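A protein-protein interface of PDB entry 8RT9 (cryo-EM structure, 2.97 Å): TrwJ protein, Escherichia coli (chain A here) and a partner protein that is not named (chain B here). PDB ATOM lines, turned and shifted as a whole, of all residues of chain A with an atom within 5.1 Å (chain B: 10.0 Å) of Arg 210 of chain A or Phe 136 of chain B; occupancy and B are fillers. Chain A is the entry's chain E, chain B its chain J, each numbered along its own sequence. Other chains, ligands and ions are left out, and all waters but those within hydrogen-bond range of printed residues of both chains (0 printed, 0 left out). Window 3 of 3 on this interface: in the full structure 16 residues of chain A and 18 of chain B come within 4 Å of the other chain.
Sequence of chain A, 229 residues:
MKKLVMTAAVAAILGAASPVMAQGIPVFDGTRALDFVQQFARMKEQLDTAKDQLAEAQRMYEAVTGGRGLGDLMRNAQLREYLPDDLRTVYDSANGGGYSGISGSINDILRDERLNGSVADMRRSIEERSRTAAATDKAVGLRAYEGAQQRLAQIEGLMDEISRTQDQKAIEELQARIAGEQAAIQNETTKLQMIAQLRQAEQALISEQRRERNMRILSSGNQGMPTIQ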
ATOM      1  N   ARG A 123       2.348  -9.166 -20.716  1.00  0.00           N
ATOM      2  CA  ARG A 123       3.197 -10.010 -21.547  1.00  0.00           C
ATOM      3  C   ARG A 123       2.372 -10.837 -22.519  1.00  0.00           C
ATOM      4  O   ARG A 123       2.696 -10.926 -23.712  1.00  0.00           O
ATOM      5  CB  ARG A 123       4.047 -10.914 -20.661  1.00  0.00           C
ATOM      6  CG  ARG A 123       4.891 -11.899 -21.416  1.00  0.00           C
ATOM      7  CD  ARG A 123       5.753 -12.708 -20.477  1.00  0.00           C
ATOM      8  NE  ARG A 123       6.266 -13.909 -21.121  1.00  0.00           N
ATOM      9  CZ  ARG A 123       6.978 -14.838 -20.498  1.00  0.00           C
ATOM     10  NH1 ARG A 123       7.270 -14.694 -19.214  1.00  0.00           N
ATOM     11  NH2 ARG A 123       7.407 -15.903 -21.158  1.00  0.00           N
ATOM     12  N   ILE A 126       0.954  -8.640 -25.278  1.00  0.00           N
ATOM     13  CA  ILE A 126       1.945  -8.194 -26.249  1.00  0.00           C
ATOM     14  C   ILE A 126       2.327  -9.328 -27.194  1.00  0.00           C
ATOM     15  O   ILE A 126       2.429  -9.129 -28.413  1.00  0.00           O
ATOM     16  CB  ILE A 126       3.170  -7.612 -25.527  1.00  0.00           C
ATOM     17  CG1 ILE A 126       2.797  -6.299 -24.850  1.00  0.00           C
ATOM     18  CG2 ILE A 126       4.298  -7.386 -26.502  1.00  0.00           C
ATOM     19  CD1 ILE A 126       3.775  -5.864 -23.805  1.00  0.00           C
ATOM     20  N   GLU A 127       2.540 -10.534 -26.659  1.00  0.00           N
ATOM     21  CA  GLU A 127       2.874 -11.662 -27.528  1.00  0.00           C
ATOM     22  C   GLU A 127       1.739 -11.978 -28.489  1.00  0.00           C
ATOM     23  O   GLU A 127       1.973 -12.266 -29.675  1.00  0.00           O
ATOM     24  CB  GLU A 127       3.222 -12.890 -26.695  1.00  0.00           C
ATOM     25  CG  GLU A 127       4.536 -12.775 -25.958  1.00  0.00           C
ATOM     26  CD  GLU A 127       4.758 -13.913 -24.992  1.00  0.00           C
ATOM     27  OE1 GLU A 127       4.282 -15.032 -25.276  1.00  0.00           O
ATOM     28  OE2 GLU A 127       5.416 -13.697 -23.953  1.00  0.00           O
ATOM     29  N   SER A 130       1.803  -9.454 -31.290  1.00  0.00           N
ATOM     30  CA  SER A 130       2.871  -9.678 -32.257  1.00  0.00           C
ATOM     31  C   SER A 130       2.509 -10.795 -33.229  1.00  0.00           C
ATOM     32  O   SER A 130       2.593 -10.629 -34.460  1.00  0.00           O
ATOM     33  CB  SER A 130       4.170  -9.991 -31.521  1.00  0.00           C
ATOM     34  OG  SER A 130       4.543  -8.920 -30.677  1.00  0.00           O
ATOM     35  N   LEU A 205       3.743   0.483 -32.458  1.00  0.00           N
ATOM     36  CA  LEU A 205       2.922   0.464 -31.253  1.00  0.00           C
ATOM     37  C   LEU A 205       3.236  -0.746 -30.383  1.00  0.00           C
ATOM     38  O   LEU A 205       3.252  -0.642 -29.150  1.00  0.00           O
ATOM     39  CB  LEU A 205       1.446   0.483 -31.630  1.00  0.00           C
ATOM     40  CG  LEU A 205       0.917   1.813 -32.153  1.00  0.00           C
ATOM     41  CD1 LEU A 205      -0.470   1.632 -32.715  1.00  0.00           C
ATOM     42  CD2 LEU A 205       0.907   2.836 -31.046  1.00  0.00           C
ATOM     43  N   ILE A 206       3.469  -1.904 -31.000  1.00  0.00           N
ATOM     44  CA  ILE A 206       3.839  -3.083 -30.221  1.00  0.00           C
ATOM     45  C   ILE A 206       5.161  -2.846 -29.504  1.00  0.00           C
ATOM     46  O   ILE A 206       5.327  -3.213 -28.332  1.00  0.00           O
ATOM     47  CB  ILE A 206       3.895  -4.329 -31.118  1.00  0.00           C
ATOM     48  CG1 ILE A 206       2.503  -4.692 -31.618  1.00  0.00           C
ATOM     49  CG2 ILE A 206       4.475  -5.499 -30.366  1.00  0.00           C
ATOM     50  CD1 ILE A 206       2.505  -5.800 -32.634  1.00  0.00           C
ATOM     51  N   SER A 207       6.121  -2.224 -30.191  1.00  0.00           N
ATOM     52  CA  SER A 207       7.384  -1.900 -29.537  1.00  0.00           C
ATOM     53  C   SER A 207       7.173  -0.938 -28.375  1.00  0.00           C
ATOM     54  O   SER A 207       7.806  -1.071 -27.318  1.00  0.00           O
ATOM     55  CB  SER A 207       8.361  -1.311 -30.549  1.00  0.00           C
ATOM     56  OG  SER A 207       9.604  -1.026 -29.936  1.00  0.00           O
ATOM     57  N   GLU A 208       6.286   0.041 -28.554  1.00  0.00           N
ATOM     58  CA  GLU A 208       6.002   0.988 -27.484  1.00  0.00           C
ATOM     59  C   GLU A 208       5.410   0.287 -26.273  1.00  0.00           C
ATOM     60  O   GLU A 208       5.754   0.606 -25.131  1.00  0.00           O
ATOM     61  CB  GLU A 208       5.048   2.071 -27.980  1.00  0.00           C
ATOM     62  CG  GLU A 208       5.644   3.027 -28.997  1.00  0.00           C
ATOM     63  CD  GLU A 208       6.804   3.847 -28.473  1.00  0.00           C
ATOM     64  OE1 GLU A 208       7.151   3.749 -27.279  1.00  0.00           O
ATOM     65  OE2 GLU A 208       7.393   4.582 -29.286  1.00  0.00           O
ATOM     66  N   GLN A 209       4.504  -0.662 -26.502  1.00  0.00           N
ATOM     67  CA  GLN A 209       3.930  -1.418 -25.392  1.00  0.00           C
ATOM     68  C   GLN A 209       4.988  -2.254 -24.688  1.00  0.00           C
ATOM     69  O   GLN A 209       4.992  -2.353 -23.452  1.00  0.00           O
ATOM     70  CB  GLN A 209       2.793  -2.298 -25.896  1.00  0.00           C
ATOM     71  CG  GLN A 209       1.494  -1.557 -26.082  1.00  0.00           C
ATOM     72  CD  GLN A 209       0.323  -2.485 -26.219  1.00  0.00           C
ATOM     73  OE1 GLN A 209       0.479  -3.639 -26.602  1.00  0.00           O
ATOM     74  NE2 GLN A 209      -0.865  -1.992 -25.905  1.00  0.00           N
ATOM     75  N   ARG A 210       5.892  -2.864 -25.455  1.00  0.00           N
ATOM     76  CA  ARG A 210       6.983  -3.609 -24.839  1.00  0.00           C
ATOM     77  C   ARG A 210       7.793  -2.710 -23.926  1.00  0.00           C
ATOM     78  O   ARG A 210       8.134  -3.090 -22.798  1.00  0.00           O
ATOM     79  CB  ARG A 210       7.903  -4.195 -25.901  1.00  0.00           C
ATOM     80  CG  ARG A 210       7.340  -5.353 -26.650  1.00  0.00           C
ATOM     81  CD  ARG A 210       8.368  -5.934 -27.586  1.00  0.00           C
ATOM     82  NE  ARG A 210       7.733  -6.748 -28.607  1.00  0.00           N
ATOM     83  CZ  ARG A 210       7.427  -8.025 -28.434  1.00  0.00           C
ATOM     84  NH1 ARG A 210       7.656  -8.593 -27.260  1.00  0.00           N
ATOM     85  NH2 ARG A 210       6.853  -8.715 -29.407  1.00  0.00           N
ATOM     86  N   ARG A 211       8.111  -1.512 -24.399  1.00  0.00           N
ATOM     87  CA  ARG A 211       8.952  -0.627 -23.610  1.00  0.00           C
ATOM     88  C   ARG A 211       8.206  -0.081 -22.403  1.00  0.00           C
ATOM     89  O   ARG A 211       8.808   0.164 -21.354  1.00  0.00           O
ATOM     90  CB  ARG A 211       9.483   0.491 -24.490  1.00  0.00           C
ATOM     91  CG  ARG A 211      10.435   1.399 -23.792  1.00  0.00           C
ATOM     92  CD  ARG A 211      10.719   2.573 -24.662  1.00  0.00           C
ATOM     93  NE  ARG A 211      11.358   2.097 -25.883  1.00  0.00           N
ATOM     94  CZ  ARG A 211      12.270   2.777 -26.556  1.00  0.00           C
ATOM     95  NH1 ARG A 211      12.667   3.947 -26.099  1.00  0.00           N
ATOM     96  NH2 ARG A 211      12.804   2.279 -27.662  1.00  0.00           N
ATOM     97  N   GLU A 212       6.894   0.102 -22.524  1.00  0.00           N
ATOM     98  CA  GLU A 212       6.106   0.488 -21.360  1.00  0.00           C
ATOM     99  C   GLU A 212       6.150  -0.592 -20.289  1.00  0.00           C
ATOM    100  O   GLU A 212       6.317  -0.291 -19.102  1.00  0.00           O
ATOM    101  CB  GLU A 212       4.665   0.770 -21.767  1.00  0.00           C
ATOM    102  CG  GLU A 212       3.794   1.243 -20.625  1.00  0.00           C
ATOM    103  CD  GLU A 212       2.372   1.538 -21.058  1.00  0.00           C
ATOM    104  OE1 GLU A 212       2.020   1.218 -22.213  1.00  0.00           O
ATOM    105  OE2 GLU A 212       1.603   2.085 -20.240  1.00  0.00           O
ATOM    106  N   ARG A 213       6.010  -1.856 -20.689  1.00  0.00           N
ATOM    107  CA  ARG A 213       6.116  -2.941 -19.718  1.00  0.00           C
ATOM    108  C   ARG A 213       7.496  -2.975 -19.082  1.00  0.00           C
ATOM    109  O   ARG A 213       7.628  -3.122 -17.858  1.00  0.00           O
ATOM    110  CB  ARG A 213       5.808  -4.276 -20.384  1.00  0.00           C
ATOM    111  CG  ARG A 213       5.696  -5.430 -19.416  1.00  0.00           C
ATOM    112  CD  ARG A 213       5.691  -6.741 -20.151  1.00  0.00           C
ATOM    113  NE  ARG A 213       5.557  -7.878 -19.254  1.00  0.00           N
ATOM    114  CZ  ARG A 213       6.547  -8.705 -18.942  1.00  0.00           C
ATOM    115  NH1 ARG A 213       7.755  -8.522 -19.448  1.00  0.00           N
ATOM    116  NH2 ARG A 213       6.329  -9.715 -18.119  1.00  0.00           N
ATOM    117  N   ASN A 214       8.538  -2.825 -19.900  1.00  0.00           N
ATOM    118  CA  ASN A 214       9.898  -2.834 -19.375  1.00  0.00           C
ATOM    119  C   ASN A 214      10.102  -1.712 -18.370  1.00  0.00           C
ATOM    120  O   ASN A 214      10.720  -1.910 -17.319  1.00  0.00           O
ATOM    121  CB  ASN A 214      10.892  -2.709 -20.523  1.00  0.00           C
ATOM    122  CG  ASN A 214      12.298  -3.013 -20.102  1.00  0.00           C
ATOM    123  OD1 ASN A 214      12.540  -3.418 -18.973  1.00  0.00           O
ATOM    124  ND2 ASN A 214      13.243  -2.814 -21.008  1.00  0.00           N
ATOM    125  N   MET A 215       9.597  -0.522 -18.708  1.00  0.00           N
ATOM    126  CA  MET A 215       9.743   0.647 -17.799  1.00  0.00           C
ATOM    127  C   MET A 215       8.990   0.363 -16.496  1.00  0.00           C
ATOM    128  O   MET A 215       9.519   0.718 -15.432  1.00  0.00           O
ATOM    129  CB  MET A 215       9.197   1.928 -18.437  1.00  0.00           C
ATOM    130  CG  MET A 215       9.937   2.354 -19.694  1.00  0.00           C
ATOM    131  SD  MET A 215      11.674   2.799 -19.420  1.00  0.00           S
ATOM    132  CE  MET A 215      12.186   3.230 -21.084  1.00  0.00           C
ATOM    133  N   SER B 128      15.404 -18.368 -13.073  1.00  0.00           N
ATOM    134  CA  SER B 128      14.748 -18.842 -14.284  1.00  0.00           C
ATOM    135  C   SER B 128      13.695 -17.857 -14.764  1.00  0.00           C
ATOM    136  O   SER B 128      13.536 -17.648 -15.970  1.00  0.00           O
ATOM    137  CB  SER B 128      14.123 -20.209 -14.035  1.00  0.00           C
ATOM    138  OG  SER B 128      13.092 -20.463 -14.966  1.00  0.00           O
ATOM    139  N   GLU B 129      12.958 -17.253 -13.837  1.00  0.00           N
ATOM    140  CA  GLU B 129      11.996 -16.229 -14.222  1.00  0.00           C
ATOM    141  C   GLU B 129      12.699 -15.023 -14.826  1.00  0.00           C
ATOM    142  O   GLU B 129      12.209 -14.425 -15.792  1.00  0.00           O
ATOM    143  CB  GLU B 129      11.159 -15.821 -13.015  1.00  0.00           C
ATOM    144  CG  GLU B 129      10.253 -16.925 -12.519  1.00  0.00           C
ATOM    145  CD  GLU B 129       9.446 -16.516 -11.312  1.00  0.00           C
ATOM    146  OE1 GLU B 129       9.684 -15.411 -10.784  1.00  0.00           O
ATOM    147  OE2 GLU B 129       8.573 -17.300 -10.888  1.00  0.00           O
ATOM    148  N   ALA B 130      13.849 -14.650 -14.268  1.00  0.00           N
ATOM    149  CA  ALA B 130      14.626 -13.568 -14.863  1.00  0.00           C
ATOM    150  C   ALA B 130      15.065 -13.920 -16.278  1.00  0.00           C
ATOM    151  O   ALA B 130      15.020 -13.077 -17.181  1.00  0.00           O
ATOM    152  CB  ALA B 130      15.837 -13.248 -13.991  1.00  0.00           C
ATOM    153  N   PHE B 131      15.496 -15.163 -16.490  1.00  0.00           N
ATOM    154  CA  PHE B 131      15.889 -15.593 -17.829  1.00  0.00           C
ATOM    155  C   PHE B 131      14.706 -15.563 -18.783  1.00  0.00           C
ATOM    156  O   PHE B 131      14.853 -15.221 -19.960  1.00  0.00           O
ATOM    157  CB  PHE B 131      16.487 -16.995 -17.777  1.00  0.00           C
ATOM    158  CG  PHE B 131      17.785 -17.070 -17.051  1.00  0.00           C
ATOM    159  CD1 PHE B 131      18.607 -15.970 -16.965  1.00  0.00           C
ATOM    160  CD2 PHE B 131      18.183 -18.242 -16.450  1.00  0.00           C
ATOM    161  CE1 PHE B 131      19.799 -16.039 -16.295  1.00  0.00           C
ATOM    162  CE2 PHE B 131      19.372 -18.315 -15.780  1.00  0.00           C
ATOM    163  CZ  PHE B 131      20.181 -17.213 -15.700  1.00  0.00           C
ATOM    164  N   GLU B 132      13.528 -15.943 -18.298  1.00  0.00           N
ATOM    165  CA  GLU B 132      12.327 -15.884 -19.120  1.00  0.00           C
ATOM    166  C   GLU B 132      12.020 -14.452 -19.533  1.00  0.00           C
ATOM    167  O   GLU B 132      11.683 -14.184 -20.692  1.00  0.00           O
ATOM    168  CB  GLU B 132      11.158 -16.488 -18.351  1.00  0.00           C
ATOM    169  CG  GLU B 132      10.052 -17.025 -19.209  1.00  0.00           C
ATOM    170  CD  GLU B 132       8.840 -17.418 -18.409  1.00  0.00           C
ATOM    171  OE1 GLU B 132       9.007 -17.821 -17.243  1.00  0.00           O
ATOM    172  OE2 GLU B 132       7.717 -17.337 -18.948  1.00  0.00           O
ATOM    173  N   GLU B 133      12.143 -13.515 -18.594  1.00  0.00           N
ATOM    174  CA  GLU B 133      11.948 -12.110 -18.932  1.00  0.00           C
ATOM    175  C   GLU B 133      12.978 -11.646 -19.946  1.00  0.00           C
ATOM    176  O   GLU B 133      12.666 -10.857 -20.845  1.00  0.00           O
ATOM    177  CB  GLU B 133      12.013 -11.251 -17.674  1.00  0.00           C
ATOM    178  CG  GLU B 133      10.791 -11.359 -16.802  1.00  0.00           C
ATOM    179  CD  GLU B 133       9.543 -10.881 -17.506  1.00  0.00           C
ATOM    180  OE1 GLU B 133       9.629  -9.892 -18.262  1.00  0.00           O
ATOM    181  OE2 GLU B 133       8.474 -11.494 -17.307  1.00  0.00           O
ATOM    182  N   ALA B 134      14.216 -12.115 -19.809  1.00  0.00           N
ATOM    183  CA  ALA B 134      15.239 -11.802 -20.800  1.00  0.00           C
ATOM    184  C   ALA B 134      14.850 -12.332 -22.168  1.00  0.00           C
ATOM    185  O   ALA B 134      15.110 -11.693 -23.190  1.00  0.00           O
ATOM    186  CB  ALA B 134      16.584 -12.381 -20.369  1.00  0.00           C
ATOM    187  N   GLY B 135      14.243 -13.513 -22.205  1.00  0.00           N
ATOM    188  CA  GLY B 135      13.777 -14.055 -23.468  1.00  0.00           C
ATOM    189  C   GLY B 135      12.661 -13.232 -24.077  1.00  0.00           C
ATOM    190  O   GLY B 135      12.573 -13.100 -25.300  1.00  0.00           O
ATOM    191  N   PHE B 136      11.789 -12.673 -23.237  1.00  0.00           N
ATOM    192  CA  PHE B 136      10.686 -11.868 -23.754  1.00  0.00           C
ATOM    193  C   PHE B 136      11.195 -10.635 -24.488  1.00  0.00           C
ATOM    194  O   PHE B 136      10.814 -10.380 -25.634  1.00  0.00           O
ATOM    195  CB  PHE B 136       9.754 -11.461 -22.618  1.00  0.00           C
ATOM    196  CG  PHE B 136       8.658 -10.537 -23.043  1.00  0.00           C
ATOM    197  CD1 PHE B 136       7.577 -11.008 -23.747  1.00  0.00           C
ATOM    198  CD2 PHE B 136       8.713  -9.196 -22.739  1.00  0.00           C
ATOM    199  CE1 PHE B 136       6.573 -10.162 -24.139  1.00  0.00           C
ATOM    200  CE2 PHE B 136       7.709  -8.348 -23.130  1.00  0.00           C
ATOM    201  CZ  PHE B 136       6.641  -8.832 -23.829  1.00  0.00           C
ATOM    202  N   PHE B 137      12.053  -9.853 -23.844  1.00  0.00           N
ATOM    203  CA  PHE B 137      12.663  -8.686 -24.476  1.00  0.00           C
ATOM    204  C   PHE B 137      13.870  -9.166 -25.265  1.00  0.00           C
ATOM    205  O   PHE B 137      14.923  -9.448 -24.691  1.00  0.00           O
ATOM    206  CB  PHE B 137      13.078  -7.657 -23.434  1.00  0.00           C
ATOM    207  CG  PHE B 137      11.977  -7.245 -22.505  1.00  0.00           C
ATOM    208  CD1 PHE B 137      11.011  -6.350 -22.911  1.00  0.00           C
ATOM    209  CD2 PHE B 137      11.918  -7.739 -21.221  1.00  0.00           C
ATOM    210  CE1 PHE B 137      10.005  -5.967 -22.056  1.00  0.00           C
ATOM    211  CE2 PHE B 137      10.914  -7.360 -20.366  1.00  0.00           C
ATOM    212  CZ  PHE B 137       9.958  -6.475 -20.784  1.00  0.00           C
ATOM    213  N   SER B 138      13.730  -9.265 -26.587  1.00  0.00           N
ATOM    214  CA  SER B 138      14.807  -9.793 -27.415  1.00  0.00           C
ATOM    215  C   SER B 138      16.075  -8.974 -27.224  1.00  0.00           C
ATOM    216  O   SER B 138      17.058  -9.463 -26.659  1.00  0.00           O
ATOM    217  CB  SER B 138      14.394  -9.805 -28.886  1.00  0.00           C
ATOM    218  OG  SER B 138      15.448 -10.266 -29.712  1.00  0.00           O
ATOM    219  N   SER B 139      16.056  -7.726 -27.664  1.00  0.00           N
ATOM    220  CA  SER B 139      17.037  -6.755 -27.216  1.00  0.00           C
ATOM    221  C   SER B 139      16.455  -5.994 -26.032  1.00  0.00           C
ATOM    222  O   SER B 139      15.256  -6.058 -25.754  1.00  0.00           O
ATOM    223  CB  SER B 139      17.417  -5.808 -28.350  1.00  0.00           C
ATOM    224  OG  SER B 139      18.014  -6.518 -29.420  1.00  0.00           O
ATOM    225  N   ASP B 140      17.318  -5.269 -25.325  1.00  0.00           N
ATOM    226  CA  ASP B 140      16.950  -4.664 -24.046  1.00  0.00           C
ATOM    227  C   ASP B 140      16.471  -5.725 -23.064  1.00  0.00           C
ATOM    228  O   ASP B 140      15.587  -5.479 -22.242  1.00  0.00           O
ATOM    229  CB  ASP B 140      15.884  -3.577 -24.219  1.00  0.00           C
ATOM    230  CG  ASP B 140      15.835  -2.614 -23.047  1.00  0.00           C
ATOM    231  OD1 ASP B 140      16.645  -2.770 -22.110  1.00  0.00           O
ATOM    232  OD2 ASP B 140      14.985  -1.699 -23.064  1.00  0.00           O
ATOM    233  N   GLY B 141      17.047  -6.917 -23.152  1.00  0.00           N
ATOM    234  CA  GLY B 141      16.633  -8.008 -22.302  1.00  0.00           C
ATOM    235  C   GLY B 141      17.794  -8.648 -21.580  1.00  0.00           C
ATOM    236  O   GLY B 141      17.595  -9.404 -20.627  1.00  0.00           O
ATOM    237  N   LEU B 142      19.017  -8.348 -22.016  1.00  0.00           N
ATOM    238  CA  LEU B 142      20.178  -8.927 -21.359  1.00  0.00           C
ATOM    239  C   LEU B 142      20.372  -8.381 -19.954  1.00  0.00           C
ATOM    240  O   LEU B 142      21.107  -8.982 -19.165  1.00  0.00           O
ATOM    241  CB  LEU B 142      21.432  -8.697 -22.191  1.00  0.00           C
ATOM    242  CG  LEU B 142      22.544  -9.698 -21.879  1.00  0.00           C
ATOM    243  CD1 LEU B 142      22.024 -11.123 -21.994  1.00  0.00           C
ATOM    244  CD2 LEU B 142      23.721  -9.489 -22.793  1.00  0.00           C
ATOM    245  N   TYR B 144      17.973  -8.452 -17.785  1.00  0.00           N
ATOM    246  CA  TYR B 144      17.353  -9.526 -17.026  1.00  0.00           C
ATOM    247  C   TYR B 144      18.236 -10.761 -16.997  1.00  0.00           C
ATOM    248  O   TYR B 144      18.228 -11.504 -16.011  1.00  0.00           O
ATOM    249  CB  TYR B 144      15.982  -9.849 -17.606  1.00  0.00           C
ATOM    250  CG  TYR B 144      15.022  -8.692 -17.540  1.00  0.00           C
ATOM    251  CD1 TYR B 144      14.965  -7.757 -18.553  1.00  0.00           C
ATOM    252  CD2 TYR B 144      14.180  -8.532 -16.458  1.00  0.00           C
ATOM    253  CE1 TYR B 144      14.095  -6.701 -18.494  1.00  0.00           C
ATOM    254  CE2 TYR B 144      13.307  -7.479 -16.391  1.00  0.00           C
ATOM    255  CZ  TYR B 144      13.268  -6.566 -17.411  1.00  0.00           C
ATOM    256  OH  TYR B 144      12.396  -5.510 -17.350  1.00  0.00           O
ATOM    257  N   GLY B 145      19.015 -10.988 -18.051  1.00  0.00           N
ATOM    258  CA  GLY B 145      19.986 -12.063 -18.013  1.00  0.00           C
ATOM    259  C   GLY B 145      21.032 -11.854 -16.938  1.00  0.00           C
ATOM    260  O   GLY B 145      21.392 -12.787 -16.221  1.00  0.00           O
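NH2 of Arg 123 of chain A lies within salt-bridge range of OE2 of Glu 132 of chain B. The guanidinium group of Arg 123 of chain A lies within salt-bridge range of the side-chain carboxylate of Glu 133 of chain B. The guanidinium group (NH1) of Arg 213 of chain A lies within salt-bridge range of the side-chain carboxylate (OE1) of Glu 133 of chain B, at 2.6 Å. The side-chain amide nitrogen of Asn 214 of chain A is in hydrogen-bond range of the side-chain carboxylate of Asp 140 of chain B (2.9 Å). The side-chain hydroxyl (OH) of Tyr 144 of chain B sits at hydrogen-bond distance from the side-chain amide oxygen (OD1) of Asn 214 of chain A (2.7 Å).
Of chain A, only Arg 123, Ile 126, Glu 127, Arg 210 and Arg 213 come within 4 Å of Phe 136 of chain B. Of chain B, only Glu 132, Glu 133 and Phe 136 come within 4 Å of Arg 123 of chain A. No residue of chain B comes within 4 Å of Ser 207 of chain A. Arg 213 of chain A touches three residues of chain B. Of the printed residues of chain A, Tyr 144 of chain B touches Asn 214 (2.7 Å). Printed residues of chain B within 4 Å of Asn 214 of chain A: Phe 137 (3.7 Å), Asp 140 (2.9 Å) and Tyr 144 (2.7 Å). Glu 129 of chain B touches none of the printed residues of chain A. The nearest printed residue of chain A that does not touch Phe 136 of chain B is Asn 214 of chain A (6.5 Å).
Among the printed residues, pairs that only touch across the chains: Arg 123 of chain A with Phe 136 of chain B, Ile 126 of chain A with Phe 136 of chain B, Glu 127 of chain A with Phe 136 of chain B, Arg 210 of chain A with Phe 136 of chain B, Arg 210 of chain A with Phe 137 of chain B, Arg 213 of chain A with Phe 136 of chain B, Arg 213 of chain A with Phe 137 of chain B and Asn 214 of chain A with Phe 137 of chain B.
The guanidinium group (NE) of Arg 123 of chain A lies within salt-bridge range of the side-chain carboxylate (OE2) of Glu 127 of chain A, 3.0 Å away. O of Ile 126 of chain A is in hydrogen-bond range of OG of Ser 130 of chain A (3.1 Å). The side-chain hydroxyl (OG) of Ser 130 of chain A lies within hydrogen-bond range of the guanidinium group (NH2) of Arg 210 of chain A (2.6 Å).
Of the 15 printed residues of chain A, 6 touch a printed residue of chain B. Printed residues of chain A that touch a printed residue of chain B: Arg 123, Ile 126, Glu 127, Arg 210, Arg 213 and Asn 214. Hydrophobic or aromatic side chains of chain A within 4 Å of the printed part of chain B: Ile 126. Printed residues of chain B that touch a printed residue of chain A: Glu 132, Glu 133, Phe 136, Phe 137, Asp 140 and Tyr 144. Hydrophobic or aromatic side chains of chain B that line the printed part of chain A: Phe 136, Phe 137 and Tyr 144. Among the printed residues, Asp or Glu carboxylates within 4 Å of a Lys or Arg side-chain nitrogen of the other chain: Arg 123 of chain A with Glu 132 of chain B, Arg 123 of chain A with Glu 133 of chain B and Arg 213 of chain A with Glu 133 of chain B.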
